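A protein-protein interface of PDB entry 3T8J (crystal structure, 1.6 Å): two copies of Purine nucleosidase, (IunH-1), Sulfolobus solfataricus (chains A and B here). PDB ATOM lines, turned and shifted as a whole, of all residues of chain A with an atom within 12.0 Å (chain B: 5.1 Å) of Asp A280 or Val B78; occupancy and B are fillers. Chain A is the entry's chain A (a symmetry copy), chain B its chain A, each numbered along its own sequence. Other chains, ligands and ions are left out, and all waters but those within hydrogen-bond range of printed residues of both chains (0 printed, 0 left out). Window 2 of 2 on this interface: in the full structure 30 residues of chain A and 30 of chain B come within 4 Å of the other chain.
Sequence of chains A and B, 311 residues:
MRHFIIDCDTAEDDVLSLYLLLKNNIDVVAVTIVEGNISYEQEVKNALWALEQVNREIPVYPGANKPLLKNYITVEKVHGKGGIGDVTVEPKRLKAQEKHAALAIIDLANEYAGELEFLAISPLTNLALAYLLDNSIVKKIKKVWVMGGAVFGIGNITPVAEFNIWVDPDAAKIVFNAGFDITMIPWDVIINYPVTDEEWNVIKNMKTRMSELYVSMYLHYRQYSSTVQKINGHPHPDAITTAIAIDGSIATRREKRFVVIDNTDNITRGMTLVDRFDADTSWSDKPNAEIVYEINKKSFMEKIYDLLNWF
The backbone carbonyl oxygen (O) of Lys B77 lies within hydrogen-bond range of a ring nitrogen (NE2) of His B220 (2.8 Å). The side-chain carboxylate (OD1) of Asp A278 lies within salt-bridge range of the guanidinium group (NH2) of Arg A276 (2.8 Å).
No position is printed for both chains. Of the 11 pairs that touch across the chains among the printed residues, none has its exchanged pair printed and touching as well.
Hydrophobic or aromatic side chains of chain B within 4 Å of the printed part of chain A: Val B78 and Tyr B224. Of the 12 printed residues of chain A, 4 touch a printed residue of chain B. Printed residues of chain A that touch a printed residue of chain B: Asp A278, Ala A279, Asp A280 and Thr A281. Hydrophobic or aromatic side chains of chain A that line the printed part of chain B: Ala A279. Among the printed residues, 11 pairs touch across the chains. Among the printed residues, no Asp or Glu carboxylate lies within 4 Å of a Lys or Arg side-chain nitrogen of the other chain.
Among the printed residues, merely in contact across the chains: Ala A279 with Asn B156, Asp A280 with Val B78, Asp A280 with Ile B157 and Ala A279 with Gln B229.
The side-chain hydroxyl (OH) of Tyr B224 sits at hydrogen-bond distance from the side-chain carboxylate (OD1) of Asp A280 (2.7 Å). The backbone carbonyl oxygen (O) of Asn B156 sits at hydrogen-bond distance from the backbone NH (N) of Asp A280, at 2.8 Å. OE1 of Gln B229 lies close to O of Asp A278. O of Asp A278 sits close to O of Val B228 (3.5 Å). The backbone carbonyl oxygen (O) of Ile B157 is in hydrogen-bond range of the side-chain hydroxyl (OG1) of Thr A281 (2.7 Å). NE2 of Gln B229 sits at hydrogen-bond distance from OD1 of Asp A280 (2.7 Å). NZ of Lys B77 lies within hydrogen-bond range of O of Asp A280.
Of the printed residues of chain B, Asp A278 touches Val B228 (3.5 Å) and Gln B229 (3.2 Å). Printed residues of chain B within 4 Å of Asp A280: Lys B77 (2.8 Å), Val B78 (3.8 Å), Asn B156 (2.8 Å), Ile B157 (3.9 Å), Tyr B224 (2.7 Å) and Gln B229 (2.7 Å). Trp A283 touches none of the printed residues of chain B. No residue of chain A comes within 4 Å of Val B75. Of chain A, only Asp A280 comes within 4 Å of Lys B77. Of the printed residues of chain A, Val B78 touches Asp A280 (3.8 Å). No residue of chain A comes within 4 Å of His B79. Ile B157 touches just these residues of chain A: Asp A280 and Thr A281. No residue of chain A comes within 4 Å of His B220. Tyr B224 touches just one residue of chain A: Asp A280 (2.7 Å). Of chain A, only Asp A278 comes within 4 Å of Val B228. Of the printed residues of chain A, Gln B229 touches Asp A278, Ala A279 and Asp A280. The nearest printed residue of chain B that does not touch Asp A280 is Val B228 (4.5 Å). The nearest printed residue of chain B that does not touch Asp A278 is Asn B156 (5.2 Å).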
ATOM      1  N   VAL A 274      21.891  23.889 -11.514  1.00  0.00           N
ATOM      2  CA  VAL A 274      23.183  23.219 -11.271  1.00  0.00           C
ATOM      3  C   VAL A 274      23.947  22.944 -12.578  1.00  0.00           C
ATOM      4  O   VAL A 274      23.463  22.220 -13.457  1.00  0.00           O
ATOM      5  CB  VAL A 274      22.979  21.923 -10.508  1.00  0.00           C
ATOM      6  CG1 VAL A 274      24.318  21.236 -10.249  1.00  0.00           C
ATOM      7  CG2 VAL A 274      22.259  22.182  -9.153  1.00  0.00           C
ATOM      8  N   ASP A 275      25.132  23.553 -12.707  1.00  0.00           N
ATOM      9  CA  ASP A 275      26.054  23.294 -13.809  1.00  0.00           C
ATOM     10  C   ASP A 275      26.903  22.089 -13.421  1.00  0.00           C
ATOM     11  O   ASP A 275      27.630  22.132 -12.414  1.00  0.00           O
ATOM     12  CB  ASP A 275      26.889  24.551 -14.071  1.00  0.00           C
ATOM     13  CG  ASP A 275      27.719  24.476 -15.360  1.00  0.00           C
ATOM     14  OD1 ASP A 275      27.851  23.383 -15.936  1.00  0.00           O
ATOM     15  OD2 ASP A 275      28.137  25.568 -15.831  1.00  0.00           O
ATOM     16  N   ARG A 276      26.816  21.032 -14.230  1.00  0.00           N
ATOM     17  CA  ARG A 276      27.539  19.776 -14.036  1.00  0.00           C
ATOM     18  C   ARG A 276      28.809  19.726 -14.905  1.00  0.00           C
ATOM     19  O   ARG A 276      29.527  18.699 -14.913  1.00  0.00           O
ATOM     20  CB  ARG A 276      26.634  18.582 -14.393  1.00  0.00           C
ATOM     21  CG  ARG A 276      25.198  18.625 -13.829  1.00  0.00           C
ATOM     22  CD  ARG A 276      24.328  17.513 -14.435  1.00  0.00           C
ATOM     23  NE  ARG A 276      24.193  17.699 -15.875  1.00  0.00           N
ATOM     24  CZ  ARG A 276      23.362  18.555 -16.463  1.00  0.00           C
ATOM     25  NH1 ARG A 276      22.510  19.276 -15.747  1.00  0.00           N
ATOM     26  NH2 ARG A 276      23.412  18.673 -17.794  1.00  0.00           N
ATOM     27  N   PHE A 277      29.067  20.801 -15.666  1.00  0.00           N
ATOM     28  CA  PHE A 277      30.226  20.918 -16.576  1.00  0.00           C
ATOM     29  C   PHE A 277      30.170  19.914 -17.745  1.00  0.00           C
ATOM     30  O   PHE A 277      31.210  19.564 -18.318  1.00  0.00           O
ATOM     31  CB  PHE A 277      31.557  20.789 -15.784  1.00  0.00           C
ATOM     32  CG  PHE A 277      31.526  21.456 -14.412  1.00  0.00           C
ATOM     33  CD1 PHE A 277      31.267  22.817 -14.286  1.00  0.00           C
ATOM     34  CD2 PHE A 277      31.737  20.726 -13.256  1.00  0.00           C
ATOM     35  CE1 PHE A 277      31.257  23.446 -13.054  1.00  0.00           C
ATOM     36  CE2 PHE A 277      31.717  21.356 -12.005  1.00  0.00           C
ATOM     37  CZ  PHE A 277      31.477  22.716 -11.910  1.00  0.00           C
ATOM     38  N   ASP A 278      28.966  19.465 -18.098  1.00  0.00           N
ATOM     39  CA  ASP A 278      28.741  18.462 -19.152  1.00  0.00           C
ATOM     40  C   ASP A 278      27.820  18.950 -20.279  1.00  0.00           C
ATOM     41  O   ASP A 278      27.344  18.155 -21.088  1.00  0.00           O
ATOM     42  CB  ASP A 278      28.152  17.170 -18.556  1.00  0.00           C
ATOM     43  CG  ASP A 278      26.745  17.342 -18.019  1.00  0.00           C
ATOM     44  OD1 ASP A 278      26.143  18.440 -18.166  1.00  0.00           O
ATOM     45  OD2 ASP A 278      26.206  16.347 -17.478  1.00  0.00           O
ATOM     46  N   ALA A 279      27.528  20.241 -20.331  1.00  0.00           N
ATOM     47  CA  ALA A 279      26.674  20.766 -21.396  1.00  0.00           C
ATOM     48  C   ALA A 279      27.475  21.494 -22.466  1.00  0.00           C
ATOM     49  O   ALA A 279      28.714  21.646 -22.341  1.00  0.00           O
ATOM     50  CB  ALA A 279      25.577  21.675 -20.789  1.00  0.00           C
ATOM     51  N   ASP A 280      26.797  21.873 -23.555  1.00  0.00           N
ATOM     52  CA  ASP A 280      27.463  22.539 -24.708  1.00  0.00           C
ATOM     53  C   ASP A 280      27.884  23.963 -24.369  1.00  0.00           C
ATOM     54  O   ASP A 280      28.735  24.540 -25.058  1.00  0.00           O
ATOM     55  CB  ASP A 280      26.537  22.560 -25.926  1.00  0.00           C
ATOM     56  CG  ASP A 280      26.104  21.170 -26.359  1.00  0.00           C
ATOM     57  OD1 ASP A 280      26.906  20.203 -26.211  1.00  0.00           O
ATOM     58  OD2 ASP A 280      24.981  21.044 -26.922  1.00  0.00           O
ATOM     59  N   THR A 281      27.280  24.535 -23.333  1.00  0.00           N
ATOM     60  CA  THR A 281      27.698  25.794 -22.747  1.00  0.00           C
ATOM     61  C   THR A 281      27.786  25.609 -21.230  1.00  0.00           C
ATOM     62  O   THR A 281      27.256  24.638 -20.664  1.00  0.00           O
ATOM     63  CB  THR A 281      26.762  26.969 -23.093  1.00  0.00           C
ATOM     64  OG1 THR A 281      25.501  26.790 -22.415  1.00  0.00           O
ATOM     65  CG2 THR A 281      26.515  27.081 -24.600  1.00  0.00           C
ATOM     66  N   SER A 282      28.471  26.532 -20.570  1.00  0.00           N
ATOM     67  CA  SER A 282      28.684  26.441 -19.127  1.00  0.00           C
ATOM     68  C   SER A 282      28.685  27.850 -18.552  1.00  0.00           C
ATOM     69  O   SER A 282      29.055  28.826 -19.223  1.00  0.00           O
ATOM     70  CB  SER A 282      29.959  25.656 -18.809  1.00  0.00           C
ATOM     71  OG  SER A 282      30.318  25.642 -17.433  1.00  0.00           O
ATOM     72  N   TRP A 283      28.201  27.967 -17.329  1.00  0.00           N
ATOM     73  CA  TRP A 283      28.088  29.255 -16.684  1.00  0.00           C
ATOM     74  C   TRP A 283      29.363  29.630 -15.934  1.00  0.00           C
ATOM     75  O   TRP A 283      29.775  30.804 -15.924  1.00  0.00           O
ATOM     76  CB  TRP A 283      26.923  29.216 -15.703  1.00  0.00           C
ATOM     77  CG  TRP A 283      25.614  28.924 -16.365  1.00  0.00           C
ATOM     78  CD1 TRP A 283      25.188  29.336 -17.597  1.00  0.00           C
ATOM     79  CD2 TRP A 283      24.526  28.175 -15.799  1.00  0.00           C
ATOM     80  NE1 TRP A 283      23.901  28.879 -17.834  1.00  0.00           N
ATOM     81  CE2 TRP A 283      23.487  28.163 -16.749  1.00  0.00           C
ATOM     82  CE3 TRP A 283      24.351  27.504 -14.589  1.00  0.00           C
ATOM     83  CZ2 TRP A 283      22.258  27.520 -16.513  1.00  0.00           C
ATOM     84  CZ3 TRP A 283      23.143  26.877 -14.346  1.00  0.00           C
ATOM     85  CH2 TRP A 283      22.112  26.891 -15.305  1.00  0.00           C
ATOM     86  N   SER A 284      29.959  28.633 -15.284  1.00  0.00           N
ATOM     87  CA  SER A 284      31.232  28.772 -14.578  1.00  0.00           C
ATOM     88  C   SER A 284      31.881  27.408 -14.466  1.00  0.00           C
ATOM     89  O   SER A 284      31.183  26.389 -14.408  1.00  0.00           O
ATOM     90  CB  SER A 284      31.057  29.348 -13.164  1.00  0.00           C
ATOM     91  OG  SER A 284      32.298  29.627 -12.526  1.00  0.00           O
ATOM     92  N   ASP A 285      33.207  27.371 -14.403  1.00  0.00           N
ATOM     93  CA  ASP A 285      33.909  26.131 -14.082  1.00  0.00           C
ATOM     94  C   ASP A 285      34.354  26.028 -12.631  1.00  0.00           C
ATOM     95  O   ASP A 285      35.108  25.128 -12.287  1.00  0.00           O
ATOM     96  CB  ASP A 285      35.099  25.959 -15.022  1.00  0.00           C
ATOM     97  CG  ASP A 285      34.674  25.451 -16.364  1.00  0.00           C
ATOM     98  OD1 ASP A 285      34.310  24.245 -16.448  1.00  0.00           O
ATOM     99  OD2 ASP A 285      34.673  26.256 -17.332  1.00  0.00           O
ATOM    100  N   VAL B  75      25.400  24.477 -33.611  1.00  0.00           N
ATOM    101  CA  VAL B  75      26.235  23.512 -32.902  1.00  0.00           C
ATOM    102  C   VAL B  75      26.943  22.511 -33.863  1.00  0.00           C
ATOM    103  O   VAL B  75      26.832  21.280 -33.731  1.00  0.00           O
ATOM    104  CB  VAL B  75      25.467  22.811 -31.765  1.00  0.00           C
ATOM    105  CG1 VAL B  75      25.288  23.793 -30.572  1.00  0.00           C
ATOM    106  CG2 VAL B  75      24.119  22.293 -32.260  1.00  0.00           C
ATOM    107  N   GLU B  76      27.678  23.056 -34.831  1.00  0.00           N
ATOM    108  CA  GLU B  76      28.475  22.208 -35.721  1.00  0.00           C
ATOM    109  C   GLU B  76      29.561  21.444 -34.948  1.00  0.00           C
ATOM    110  O   GLU B  76      30.029  20.408 -35.425  1.00  0.00           O
ATOM    111  CB  GLU B  76      29.026  23.011 -36.915  1.00  0.00           C
ATOM    112  CG  GLU B  76      27.894  23.413 -37.893  1.00  0.00           C
ATOM    113  CD  GLU B  76      28.210  24.601 -38.793  1.00  0.00           C
ATOM    114  OE1 GLU B  76      29.398  24.907 -38.998  1.00  0.00           O
ATOM    115  OE2 GLU B  76      27.256  25.233 -39.310  1.00  0.00           O
ATOM    116  N   LYS B  77      29.942  21.908 -33.752  1.00  0.00           N
ATOM    117  CA  LYS B  77      30.866  21.123 -32.914  1.00  0.00           C
ATOM    118  C   LYS B  77      30.243  19.767 -32.525  1.00  0.00           C
ATOM    119  O   LYS B  77      30.944  18.765 -32.336  1.00  0.00           O
ATOM    120  CB  LYS B  77      31.328  21.914 -31.678  1.00  0.00           C
ATOM    121  CG  LYS B  77      30.249  22.181 -30.616  1.00  0.00           C
ATOM    122  CD  LYS B  77      30.767  23.018 -29.469  1.00  0.00           C
ATOM    123  CE  LYS B  77      29.697  23.352 -28.433  1.00  0.00           C
ATOM    124  NZ  LYS B  77      30.311  24.148 -27.302  1.00  0.00           N
ATOM    125  N   VAL B  78      28.911  19.755 -32.363  1.00  0.00           N
ATOM    126  CA  VAL B  78      28.206  18.567 -31.936  1.00  0.00           C
ATOM    127  C   VAL B  78      27.956  17.610 -33.103  1.00  0.00           C
ATOM    128  O   VAL B  78      28.126  16.398 -32.955  1.00  0.00           O
ATOM    129  CB  VAL B  78      26.832  18.969 -31.290  1.00  0.00           C
ATOM    130  CG1 VAL B  78      25.998  17.721 -30.943  1.00  0.00           C
ATOM    131  CG2 VAL B  78      27.020  19.853 -30.033  1.00  0.00           C
ATOM    132  N   HIS B  79      27.547  18.145 -34.253  1.00  0.00           N
ATOM    133  CA  HIS B  79      27.048  17.331 -35.387  1.00  0.00           C
ATOM    134  C   HIS B  79      27.980  17.290 -36.599  1.00  0.00           C
ATOM    135  O   HIS B  79      27.689  16.587 -37.561  1.00  0.00           O
ATOM    136  CB  HIS B  79      25.676  17.850 -35.868  1.00  0.00           C
ATOM    137  CG  HIS B  79      24.633  17.885 -34.799  1.00  0.00           C
ATOM    138  ND1 HIS B  79      23.928  16.762 -34.411  1.00  0.00           N
ATOM    139  CD2 HIS B  79      24.184  18.899 -34.022  1.00  0.00           C
ATOM    140  CE1 HIS B  79      23.092  17.086 -33.438  1.00  0.00           C
ATOM    141  NE2 HIS B  79      23.234  18.375 -33.173  1.00  0.00           N
ATOM    142  N   GLY B  80      29.072  18.037 -36.564  1.00  0.00           N
ATOM    143  CA  GLY B  80      29.927  18.244 -37.746  1.00  0.00           C
ATOM    144  C   GLY B  80      29.460  19.418 -38.592  1.00  0.00           C
ATOM    145  O   GLY B  80      28.299  19.820 -38.523  1.00  0.00           O
ATOM    146  N   ASN B 156      21.079  19.976 -22.434  1.00  0.00           N
ATOM    147  CA  ASN B 156      22.244  19.788 -23.323  1.00  0.00           C
ATOM    148  C   ASN B 156      22.884  21.096 -23.783  1.00  0.00           C
ATOM    149  O   ASN B 156      24.100  21.281 -23.636  1.00  0.00           O
ATOM    150  CB  ASN B 156      21.953  18.819 -24.485  1.00  0.00           C
ATOM    151  CG  ASN B 156      20.805  19.220 -25.414  1.00  0.00           C
ATOM    152  OD1 ASN B 156      20.073  20.179 -25.186  1.00  0.00           O
ATOM    153  ND2 ASN B 156      20.648  18.455 -26.501  1.00  0.00           N
ATOM    154  N   ILE B 157      22.086  22.032 -24.284  1.00  0.00           N
ATOM    155  CA  ILE B 157      22.644  23.298 -24.775  1.00  0.00           C
ATOM    156  C   ILE B 157      23.102  24.189 -23.617  1.00  0.00           C
ATOM    157  O   ILE B 157      24.122  24.863 -23.732  1.00  0.00           O
ATOM    158  CB  ILE B 157      21.650  24.033 -25.727  1.00  0.00           C
ATOM    159  CG1 ILE B 157      22.321  25.248 -26.382  1.00  0.00           C
ATOM    160  CG2 ILE B 157      20.309  24.407 -25.021  1.00  0.00           C
ATOM    161  CD1 ILE B 157      23.557  24.954 -27.248  1.00  0.00           C
ATOM    162  N   HIS B 220      30.899  11.260 -35.751  1.00  0.00           N
ATOM    163  CA  HIS B 220      31.292  12.530 -35.095  1.00  0.00           C
ATOM    164  C   HIS B 220      30.420  12.793 -33.870  1.00  0.00           C
ATOM    165  O   HIS B 220      30.933  13.126 -32.812  1.00  0.00           O
ATOM    166  CB  HIS B 220      31.217  13.715 -36.092  1.00  0.00           C
ATOM    167  CG  HIS B 220      31.562  15.049 -35.492  1.00  0.00           C
ATOM    168  ND1 HIS B 220      32.687  15.765 -35.841  1.00  0.00           N
ATOM    169  CD2 HIS B 220      30.908  15.808 -34.577  1.00  0.00           C
ATOM    170  CE1 HIS B 220      32.732  16.890 -35.145  1.00  0.00           C
ATOM    171  NE2 HIS B 220      31.654  16.941 -34.374  1.00  0.00           N
ATOM    172  N   TYR B 221      29.103  12.637 -34.035  1.00  0.00           N
ATOM    173  CA  TYR B 221      28.135  12.839 -32.956  1.00  0.00           C
ATOM    174  C   TYR B 221      28.376  11.902 -31.780  1.00  0.00           C
ATOM    175  O   TYR B 221      28.287  12.312 -30.617  1.00  0.00           O
ATOM    176  CB  TYR B 221      26.731  12.608 -33.510  1.00  0.00           C
ATOM    177  CG  TYR B 221      25.549  12.905 -32.605  1.00  0.00           C
ATOM    178  CD1 TYR B 221      25.394  14.145 -32.024  1.00  0.00           C
ATOM    179  CD2 TYR B 221      24.530  11.959 -32.424  1.00  0.00           C
ATOM    180  CE1 TYR B 221      24.257  14.438 -31.248  1.00  0.00           C
ATOM    181  CE2 TYR B 221      23.396  12.257 -31.663  1.00  0.00           C
ATOM    182  CZ  TYR B 221      23.283  13.488 -31.081  1.00  0.00           C
ATOM    183  OH  TYR B 221      22.164  13.803 -30.321  1.00  0.00           O
ATOM    184  N   TYR B 224      31.448  13.074 -29.778  1.00  0.00           N
ATOM    185  CA  TYR B 224      31.175  14.272 -29.006  1.00  0.00           C
ATOM    186  C   TYR B 224      30.279  13.921 -27.826  1.00  0.00           C
ATOM    187  O   TYR B 224      30.505  14.362 -26.694  1.00  0.00           O
ATOM    188  CB  TYR B 224      30.491  15.335 -29.869  1.00  0.00           C
ATOM    189  CG  TYR B 224      30.209  16.603 -29.118  1.00  0.00           C
ATOM    190  CD1 TYR B 224      31.099  17.657 -29.131  1.00  0.00           C
ATOM    191  CD2 TYR B 224      29.025  16.750 -28.391  1.00  0.00           C
ATOM    192  CE1 TYR B 224      30.865  18.814 -28.430  1.00  0.00           C
ATOM    193  CE2 TYR B 224      28.781  17.901 -27.683  1.00  0.00           C
ATOM    194  CZ  TYR B 224      29.682  18.935 -27.714  1.00  0.00           C
ATOM    195  OH  TYR B 224      29.438  20.097 -27.023  1.00  0.00           O
ATOM    196  N   VAL B 228      31.844  14.836 -24.146  1.00  0.00           N
ATOM    197  CA  VAL B 228      31.374  16.086 -23.541  1.00  0.00           C
ATOM    198  C   VAL B 228      30.186  15.860 -22.636  1.00  0.00           C
ATOM    199  O   VAL B 228      30.195  16.236 -21.456  1.00  0.00           O
ATOM    200  CB  VAL B 228      31.001  17.125 -24.623  1.00  0.00           C
ATOM    201  CG1 VAL B 228      30.432  18.398 -24.005  1.00  0.00           C
ATOM    202  CG2 VAL B 228      32.222  17.442 -25.463  1.00  0.00           C
ATOM    203  N   GLN B 229      29.157  15.232 -23.191  1.00  0.00           N
ATOM    204  CA  GLN B 229      27.904  15.005 -22.491  1.00  0.00           C
ATOM    205  C   GLN B 229      27.989  13.789 -21.558  1.00  0.00           C
ATOM    206  O   GLN B 229      27.106  13.564 -20.719  1.00  0.00           O
ATOM    207  CB  GLN B 229      26.778  14.832 -23.521  1.00  0.00           C
ATOM    208  CG  GLN B 229      26.649  16.010 -24.520  1.00  0.00           C
ATOM    209  CD  GLN B 229      25.869  17.154 -23.913  1.00  0.00           C
ATOM    210  OE1 GLN B 229      25.087  16.949 -22.982  1.00  0.00           O
ATOM    211  NE2 GLN B 229      26.090  18.364 -24.411  1.00  0.00           N
